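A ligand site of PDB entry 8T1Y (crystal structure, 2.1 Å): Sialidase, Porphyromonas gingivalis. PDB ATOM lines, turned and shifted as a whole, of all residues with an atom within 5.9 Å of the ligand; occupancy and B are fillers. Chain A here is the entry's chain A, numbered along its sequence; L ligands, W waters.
The guanidinium group of Arg 177 lies within salt-bridge range of an oxygen (O1) of the ligand (2.7 Å). The side-chain carboxylate (OD1) of Asp 364 is in hydrogen-bond range of an oxygen (O6) of the ligand (2.7 Å). OD2 of Asp 239 lies within hydrogen-bond range of N1 of the ligand (2.8 Å). The guanidinium group (NH1) of Arg 443 lies within salt-bridge range of an oxygen (O1) of the ligand (2.8 Å). OH of Tyr 471 lies close to O4 of the ligand. NH2 of Arg 196 lies within hydrogen-bond range of O3 of the ligand (2.9 Å). The guanidinium group (NH2) of Arg 381 lies within salt-bridge range of an oxygen (O2) of the ligand. OD1 of Asp 202 is in hydrogen-bond range of O3 of the ligand (3.3 Å). An oxygen (O6) of the ligand lies close to the side-chain carboxylate of Glu 365 (3.5 Å).
The side-chain carboxylate of Glu 487 is in salt-bridge range of the guanidinium group of Arg 177 (2.8 Å). The guanidinium group (NE) of Arg 381 is in salt-bridge range of the side-chain carboxylate (OD1) of Asp 364. The guanidinium group (NH2) of Arg 443 sits at hydrogen-bond distance from the backbone carbonyl oxygen (O) of Gly 416, 2.7 Å away. The backbone NH (N) of Tyr 471 sits at hydrogen-bond distance from the side-chain carboxylate (OE1) of Glu 487 (2.8 Å). OD1 of Asp 202 is in salt-bridge range of NH1 of Arg 196, 3.0 Å away. The guanidinium group of Arg 196 is in salt-bridge range of the side-chain carboxylate of Asp 194. The guanidinium group (NH1) of Arg 381 is in salt-bridge range of the side-chain carboxylate (OE1) of Glu 365. N of Ile 178 lies within hydrogen-bond range of OE2 of Glu 487, 2.8 Å away.
Ile 178 touches the ligand (CD1 to O3, 3.5 Å). Leu 260 touches the ligand. Phe 310 touches the ligand (CZ to O6, 3.5 Å). CG of Gln 383 touches O7 of the ligand (3.9 Å). Hydrophobic or aromatic side chains within 4 Å of the ligand: Ile 178, Leu 260, Phe 310 and Tyr 471. Within 4 Å of the ligand: Arg 177, Ile 178, Arg 196, Asp 202, Asp 239, Leu 260, Phe 310, Asp 364, Glu 365, Arg 381, Gln 383, Arg 443 and Tyr 471.
Water W1 lies within hydrogen-bond range of OD2 of Asp 202 (2.7 Å) and O4 of the ligand (2.7 Å). Water W4 lies within hydrogen-bond range of O8 of the ligand (2.8 Å), N of Leu 260 (2.9 Å) and O of Leu 203 (3.1 Å). Water W3 lies within hydrogen-bond range of an oxygen (O5) of the ligand (3.0 Å) and the indole nitrogen of Trp 261 (3.1 Å). Water W5 bridges the backbone NH of Leu 203 (2.9 Å) and an oxygen (O3) of the ligand (3.2 Å).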
ATOM      1  N   ARG A 177      11.740  20.151  38.367  1.00  0.00           N
ATOM      2  CA  ARG A 177      10.682  19.398  37.707  1.00  0.00           C
ATOM      3  C   ARG A 177      11.307  18.486  36.656  1.00  0.00           C
ATOM      4  O   ARG A 177      12.499  18.603  36.321  1.00  0.00           O
ATOM      5  CB  ARG A 177       9.644  20.327  37.057  1.00  0.00           C
ATOM      6  CG  ARG A 177       8.545  20.823  38.010  1.00  0.00           C
ATOM      7  CD  ARG A 177       7.216  21.000  37.314  1.00  0.00           C
ATOM      8  NE  ARG A 177       6.667  19.716  36.862  1.00  0.00           N
ATOM      9  CZ  ARG A 177       5.772  19.598  35.896  1.00  0.00           C
ATOM     10  NH1 ARG A 177       5.293  20.648  35.249  1.00  0.00           N
ATOM     11  NH2 ARG A 177       5.325  18.384  35.562  1.00  0.00           N
ATOM     12  N   ILE A 178      10.482  17.584  36.128  1.00  0.00           N
ATOM     13  CA  ILE A 178      10.721  16.833  34.894  1.00  0.00           C
ATOM     14  C   ILE A 178      11.830  15.798  35.099  1.00  0.00           C
ATOM     15  O   ILE A 178      12.944  15.954  34.567  1.00  0.00           O
ATOM     16  CB  ILE A 178      11.046  17.756  33.700  1.00  0.00           C
ATOM     17  CG1 ILE A 178      10.223  19.064  33.706  1.00  0.00           C
ATOM     18  CG2 ILE A 178      10.770  17.021  32.391  1.00  0.00           C
ATOM     19  CD1 ILE A 178       8.736  18.901  33.674  1.00  0.00           C
ATOM     20  N   ASP A 194      14.788  19.240  35.090  1.00  0.00           N
ATOM     21  CA  ASP A 194      14.663  20.692  34.941  1.00  0.00           C
ATOM     22  C   ASP A 194      15.105  21.355  36.250  1.00  0.00           C
ATOM     23  O   ASP A 194      14.487  21.146  37.307  1.00  0.00           O
ATOM     24  CB  ASP A 194      13.222  21.110  34.641  1.00  0.00           C
ATOM     25  CG  ASP A 194      12.841  21.069  33.159  1.00  0.00           C
ATOM     26  OD1 ASP A 194      13.406  20.261  32.401  1.00  0.00           O
ATOM     27  OD2 ASP A 194      11.928  21.846  32.765  1.00  0.00           O
ATOM     28  N   ARG A 196      14.535  24.506  37.670  1.00  0.00           N
ATOM     29  CA  ARG A 196      13.603  25.595  37.355  1.00  0.00           C
ATOM     30  C   ARG A 196      13.909  26.756  38.295  1.00  0.00           C
ATOM     31  O   ARG A 196      13.399  26.852  39.405  1.00  0.00           O
ATOM     32  CB  ARG A 196      12.171  25.097  37.430  1.00  0.00           C
ATOM     33  CG  ARG A 196      11.879  23.995  36.417  1.00  0.00           C
ATOM     34  CD  ARG A 196      10.442  24.002  35.909  1.00  0.00           C
ATOM     35  NE  ARG A 196      10.271  23.171  34.716  1.00  0.00           N
ATOM     36  CZ  ARG A 196       9.111  22.938  34.110  1.00  0.00           C
ATOM     37  NH1 ARG A 196       7.971  23.387  34.601  1.00  0.00           N
ATOM     38  NH2 ARG A 196       9.104  22.257  32.970  1.00  0.00           N
ATOM     39  N   ASP A 202       6.782  26.263  32.964  1.00  0.00           N
ATOM     40  CA  ASP A 202       7.440  25.659  31.809  1.00  0.00           C
ATOM     41  C   ASP A 202       8.339  26.658  31.059  1.00  0.00           C
ATOM     42  O   ASP A 202       8.411  27.842  31.396  1.00  0.00           O
ATOM     43  CB  ASP A 202       6.407  25.112  30.814  1.00  0.00           C
ATOM     44  CG  ASP A 202       5.533  24.003  31.402  1.00  0.00           C
ATOM     45  OD1 ASP A 202       5.966  23.302  32.347  1.00  0.00           O
ATOM     46  OD2 ASP A 202       4.412  23.793  30.862  1.00  0.00           O
ATOM     47  N   LEU A 203       9.030  26.178  30.029  1.00  0.00           N
ATOM     48  CA  LEU A 203       9.544  27.113  29.030  1.00  0.00           C
ATOM     49  C   LEU A 203       8.372  27.942  28.512  1.00  0.00           C
ATOM     50  O   LEU A 203       7.263  27.403  28.360  1.00  0.00           O
ATOM     51  CB  LEU A 203      10.231  26.362  27.889  1.00  0.00           C
ATOM     52  CG  LEU A 203      11.423  25.450  28.208  1.00  0.00           C
ATOM     53  CD1 LEU A 203      11.700  24.545  27.025  1.00  0.00           C
ATOM     54  CD2 LEU A 203      12.676  26.246  28.551  1.00  0.00           C
ATOM     55  N   ASP A 239      13.141  19.449  29.520  1.00  0.00           N
ATOM     56  CA  ASP A 239      12.434  18.246  29.059  1.00  0.00           C
ATOM     57  C   ASP A 239      13.399  17.209  28.463  1.00  0.00           C
ATOM     58  O   ASP A 239      13.420  16.946  27.262  1.00  0.00           O
ATOM     59  CB  ASP A 239      11.330  18.638  28.073  1.00  0.00           C
ATOM     60  CG  ASP A 239      10.020  18.996  28.783  1.00  0.00           C
ATOM     61  OD1 ASP A 239      10.050  19.766  29.782  1.00  0.00           O
ATOM     62  OD2 ASP A 239       8.954  18.521  28.341  1.00  0.00           O
ATOM     63  N   VAL A 255      14.659  20.048  24.661  1.00  0.00           N
ATOM     64  CA  VAL A 255      14.242  21.251  23.940  1.00  0.00           C
ATOM     65  C   VAL A 255      14.779  22.498  24.633  1.00  0.00           C
ATOM     66  O   VAL A 255      15.304  22.451  25.755  1.00  0.00           O
ATOM     67  CB  VAL A 255      12.708  21.344  23.767  1.00  0.00           C
ATOM     68  CG1 VAL A 255      12.215  20.267  22.806  1.00  0.00           C
ATOM     69  CG2 VAL A 255      11.977  21.305  25.078  1.00  0.00           C
ATOM     70  N   LEU A 260       6.178  25.809  23.970  1.00  0.00           N
ATOM     71  CA  LEU A 260       5.652  24.868  22.981  1.00  0.00           C
ATOM     72  C   LEU A 260       4.651  25.544  22.036  1.00  0.00           C
ATOM     73  O   LEU A 260       4.780  25.432  20.814  1.00  0.00           O
ATOM     74  CB  LEU A 260       5.011  23.683  23.707  1.00  0.00           C
ATOM     75  CG  LEU A 260       4.401  22.546  22.894  1.00  0.00           C
ATOM     76  CD1 LEU A 260       5.464  21.891  21.999  1.00  0.00           C
ATOM     77  CD2 LEU A 260       3.785  21.495  23.801  1.00  0.00           C
ATOM     78  N   TRP A 261       3.691  26.265  22.584  1.00  0.00           N
ATOM     79  CA  TRP A 261       2.684  26.939  21.769  1.00  0.00           C
ATOM     80  C   TRP A 261       3.147  28.293  21.204  1.00  0.00           C
ATOM     81  O   TRP A 261       2.392  28.907  20.443  1.00  0.00           O
ATOM     82  CB  TRP A 261       1.396  27.112  22.578  1.00  0.00           C
ATOM     83  CG  TRP A 261       1.015  25.806  23.237  1.00  0.00           C
ATOM     84  CD1 TRP A 261       1.164  25.468  24.558  1.00  0.00           C
ATOM     85  CD2 TRP A 261       0.502  24.632  22.583  1.00  0.00           C
ATOM     86  NE1 TRP A 261       0.747  24.179  24.768  1.00  0.00           N
ATOM     87  CE2 TRP A 261       0.345  23.638  23.576  1.00  0.00           C
ATOM     88  CE3 TRP A 261       0.153  24.330  21.258  1.00  0.00           C
ATOM     89  CZ2 TRP A 261      -0.170  22.361  23.285  1.00  0.00           C
ATOM     90  CZ3 TRP A 261      -0.339  23.058  20.971  1.00  0.00           C
ATOM     91  CH2 TRP A 261      -0.497  22.088  21.983  1.00  0.00           C
ATOM     92  N   GLN A 269      10.948  26.584  18.917  1.00  0.00           N
ATOM     93  CA  GLN A 269      11.585  25.965  20.061  1.00  0.00           C
ATOM     94  C   GLN A 269      12.329  24.727  19.567  1.00  0.00           C
ATOM     95  O   GLN A 269      11.734  23.858  18.928  1.00  0.00           O
ATOM     96  CB  GLN A 269      10.529  25.591  21.108  1.00  0.00           C
ATOM     97  CG  GLN A 269      10.947  24.542  22.117  1.00  0.00           C
ATOM     98  CD  GLN A 269       9.759  23.977  22.856  1.00  0.00           C
ATOM     99  OE1 GLN A 269       9.081  23.081  22.356  1.00  0.00           O
ATOM    100  NE2 GLN A 269       9.481  24.515  24.056  1.00  0.00           N
ATOM    101  N   PHE A 310       8.386  18.320  20.478  1.00  0.00           N
ATOM    102  CA  PHE A 310       9.193  17.935  21.628  1.00  0.00           C
ATOM    103  C   PHE A 310       9.055  16.452  21.928  1.00  0.00           C
ATOM    104  O   PHE A 310       7.981  15.867  21.792  1.00  0.00           O
ATOM    105  CB  PHE A 310       8.885  18.773  22.873  1.00  0.00           C
ATOM    106  CG  PHE A 310       7.655  18.345  23.656  1.00  0.00           C
ATOM    107  CD1 PHE A 310       6.372  18.540  23.154  1.00  0.00           C
ATOM    108  CD2 PHE A 310       7.783  17.874  24.960  1.00  0.00           C
ATOM    109  CE1 PHE A 310       5.249  18.190  23.911  1.00  0.00           C
ATOM    110  CE2 PHE A 310       6.672  17.544  25.721  1.00  0.00           C
ATOM    111  CZ  PHE A 310       5.395  17.704  25.193  1.00  0.00           C
ATOM    112  N   LEU A 339      -1.629  18.123  19.249  1.00  0.00           N
ATOM    113  CA  LEU A 339      -0.353  17.581  18.793  1.00  0.00           C
ATOM    114  C   LEU A 339      -0.583  16.214  18.178  1.00  0.00           C
ATOM    115  O   LEU A 339      -1.556  15.538  18.488  1.00  0.00           O
ATOM    116  CB  LEU A 339       0.658  17.489  19.960  1.00  0.00           C
ATOM    117  CG  LEU A 339       0.883  18.730  20.848  1.00  0.00           C
ATOM    118  CD1 LEU A 339       1.624  18.367  22.137  1.00  0.00           C
ATOM    119  CD2 LEU A 339       1.660  19.805  20.108  1.00  0.00           C
ATOM    120  N   ASP A 364       0.018  13.349  22.716  1.00  0.00           N
ATOM    121  CA  ASP A 364       0.838  14.176  23.583  1.00  0.00           C
ATOM    122  C   ASP A 364       2.050  13.335  23.991  1.00  0.00           C
ATOM    123  O   ASP A 364       2.445  12.428  23.255  1.00  0.00           O
ATOM    124  CB  ASP A 364       0.027  14.651  24.783  1.00  0.00           C
ATOM    125  CG  ASP A 364       0.505  16.020  25.309  1.00  0.00           C
ATOM    126  OD1 ASP A 364       1.536  16.045  26.017  1.00  0.00           O
ATOM    127  OD2 ASP A 364      -0.153  17.053  25.040  1.00  0.00           O
ATOM    128  N   GLU A 365       2.630  13.613  25.169  1.00  0.00           N
ATOM    129  CA  GLU A 365       3.834  12.893  25.628  1.00  0.00           C
ATOM    130  C   GLU A 365       3.640  11.377  25.543  1.00  0.00           C
ATOM    131  O   GLU A 365       2.739  10.836  26.180  1.00  0.00           O
ATOM    132  CB  GLU A 365       4.147  13.300  27.066  1.00  0.00           C
ATOM    133  CG  GLU A 365       4.907  14.625  27.213  1.00  0.00           C
ATOM    134  CD  GLU A 365       4.810  15.189  28.635  1.00  0.00           C
ATOM    135  OE1 GLU A 365       3.968  14.678  29.420  1.00  0.00           O
ATOM    136  OE2 GLU A 365       5.570  16.128  28.965  1.00  0.00           O
ATOM    137  N   ARG A 381      -0.024   9.994  26.394  1.00  0.00           N
ATOM    138  CA  ARG A 381      -0.693  10.869  27.339  1.00  0.00           C
ATOM    139  C   ARG A 381      -2.017  11.383  26.787  1.00  0.00           C
ATOM    140  O   ARG A 381      -2.107  11.783  25.617  1.00  0.00           O
ATOM    141  CB  ARG A 381       0.210  12.048  27.676  1.00  0.00           C
ATOM    142  CG  ARG A 381      -0.409  13.136  28.519  1.00  0.00           C
ATOM    143  CD  ARG A 381       0.665  14.107  28.994  1.00  0.00           C
ATOM    144  NE  ARG A 381       0.140  15.451  29.225  1.00  0.00           N
ATOM    145  CZ  ARG A 381       0.737  16.358  29.990  1.00  0.00           C
ATOM    146  NH1 ARG A 381       1.908  16.121  30.558  1.00  0.00           N
ATOM    147  NH2 ARG A 381       0.157  17.550  30.165  1.00  0.00           N
ATOM    148  N   GLN A 383      -4.210  14.196  26.656  1.00  0.00           N
ATOM    149  CA  GLN A 383      -4.237  15.635  26.915  1.00  0.00           C
ATOM    150  C   GLN A 383      -5.604  16.200  26.526  1.00  0.00           C
ATOM    151  O   GLN A 383      -6.027  16.049  25.375  1.00  0.00           O
ATOM    152  CB  GLN A 383      -3.142  16.365  26.129  1.00  0.00           C
ATOM    153  CG  GLN A 383      -2.980  17.842  26.479  1.00  0.00           C
ATOM    154  CD  GLN A 383      -2.820  18.080  27.973  1.00  0.00           C
ATOM    155  OE1 GLN A 383      -2.023  17.416  28.650  1.00  0.00           O
ATOM    156  NE2 GLN A 383      -3.544  19.041  28.499  1.00  0.00           N
ATOM    157  N   GLY A 416      -3.850  13.231  32.633  1.00  0.00           N
ATOM    158  CA  GLY A 416      -3.214  14.109  31.687  1.00  0.00           C
ATOM    159  C   GLY A 416      -1.794  14.410  32.103  1.00  0.00           C
ATOM    160  O   GLY A 416      -1.450  15.556  32.397  1.00  0.00           O
ATOM    161  N   ARG A 443      -3.344  15.458  39.614  1.00  0.00           N
ATOM    162  CA  ARG A 443      -2.010  14.892  39.734  1.00  0.00           C
ATOM    163  C   ARG A 443      -1.782  14.539  41.207  1.00  0.00           C
ATOM    164  O   ARG A 443      -1.207  15.290  41.999  1.00  0.00           O
ATOM    165  CB  ARG A 443      -0.965  15.837  39.163  1.00  0.00           C
ATOM    166  CG  ARG A 443      -0.921  15.738  37.626  1.00  0.00           C
ATOM    167  CD  ARG A 443      -0.158  16.883  37.000  1.00  0.00           C
ATOM    168  NE  ARG A 443      -0.284  16.839  35.544  1.00  0.00           N
ATOM    169  CZ  ARG A 443       0.575  17.413  34.714  1.00  0.00           C
ATOM    170  NH1 ARG A 443       1.624  18.096  35.147  1.00  0.00           N
ATOM    171  NH2 ARG A 443       0.355  17.323  33.393  1.00  0.00           N
ATOM    172  N   TYR A 471       4.958  13.811  37.272  1.00  0.00           N
ATOM    173  CA  TYR A 471       5.752  13.064  36.313  1.00  0.00           C
ATOM    174  C   TYR A 471       6.507  11.961  37.019  1.00  0.00           C
ATOM    175  O   TYR A 471       6.962  12.135  38.163  1.00  0.00           O
ATOM    176  CB  TYR A 471       6.734  13.968  35.582  1.00  0.00           C
ATOM    177  CG  TYR A 471       6.121  14.738  34.438  1.00  0.00           C
ATOM    178  CD1 TYR A 471       4.783  15.096  34.443  1.00  0.00           C
ATOM    179  CD2 TYR A 471       6.901  15.118  33.360  1.00  0.00           C
ATOM    180  CE1 TYR A 471       4.227  15.796  33.396  1.00  0.00           C
ATOM    181  CE2 TYR A 471       6.352  15.816  32.305  1.00  0.00           C
ATOM    182  CZ  TYR A 471       5.024  16.143  32.327  1.00  0.00           C
ATOM    183  OH  TYR A 471       4.492  16.819  31.280  1.00  0.00           O
ATOM    184  N   GLU A 487       7.846  13.042  40.731  1.00  0.00           N
ATOM    185  CA  GLU A 487       7.598  14.418  41.197  1.00  0.00           C
ATOM    186  C   GLU A 487       6.653  14.403  42.390  1.00  0.00           C
ATOM    187  O   GLU A 487       5.447  14.251  42.230  1.00  0.00           O
ATOM    188  CB  GLU A 487       6.987  15.264  40.087  1.00  0.00           C
ATOM    189  CG  GLU A 487       7.792  15.333  38.801  1.00  0.00           C
ATOM    190  CD  GLU A 487       7.287  16.429  37.865  1.00  0.00           C
ATOM    191  OE1 GLU A 487       6.104  16.363  37.470  1.00  0.00           O
ATOM    192  OE2 GLU A 487       8.063  17.355  37.530  1.00  0.00           O
HETATM  193  C1  LIG L   1       3.259  19.437  32.398  1.00  0.00           C
HETATM  194  C2  LIG L   1       4.250  19.669  31.353  1.00  0.00           C
HETATM  195  C3  LIG L   1       5.564  19.776  31.630  1.00  0.00           C
HETATM  196  C4  LIG L   1       6.595  19.973  30.536  1.00  0.00           C
HETATM  197  C5  LIG L   1       5.911  20.438  29.250  1.00  0.00           C
HETATM  198  C6  LIG L   1       4.713  19.538  28.971  1.00  0.00           C
HETATM  199  C7  LIG L   1       3.989  19.975  27.714  1.00  0.00           C
HETATM  200  C8  LIG L   1       2.658  19.238  27.543  1.00  0.00           C
HETATM  201  C9  LIG L   1       1.983  19.584  26.220  1.00  0.00           C
HETATM  202  C10 LIG L   1       6.948  21.374  27.271  1.00  0.00           C
HETATM  203  C11 LIG L   1       8.106  21.319  26.317  1.00  0.00           C
HETATM  204  N1  LIG L   1       6.844  20.364  28.140  1.00  0.00           N
HETATM  205  O1  LIG L   1       3.627  19.338  33.591  1.00  0.00           O
HETATM  206  O2  LIG L   1       2.052  19.256  32.098  1.00  0.00           O
HETATM  207  O3  LIG L   1       7.666  20.851  30.929  1.00  0.00           O
HETATM  208  O4  LIG L   1       3.752  19.712  30.014  1.00  0.00           O
HETATM  209  O5  LIG L   1       3.716  21.388  27.827  1.00  0.00           O
HETATM  210  O6  LIG L   1       2.888  17.837  27.604  1.00  0.00           O
HETATM  211  O7  LIG L   1       0.573  19.445  26.392  1.00  0.00           O
HETATM  212  O8  LIG L   1       6.132  22.287  27.253  1.00  0.00           O
HETATM  213  O   HOH W   1       2.465  22.114  30.162  1.00  0.00           O
HETATM  214  O   HOH W   2      -1.179  21.513  27.053  1.00  0.00           O
HETATM  215  O   HOH W   3       1.289  23.225  27.671  1.00  0.00           O
HETATM  216  O   HOH W   4       6.895  24.911  26.628  1.00  0.00           O
HETATM  217  O   HOH W   5       8.871  23.311  29.359  1.00  0.00           O
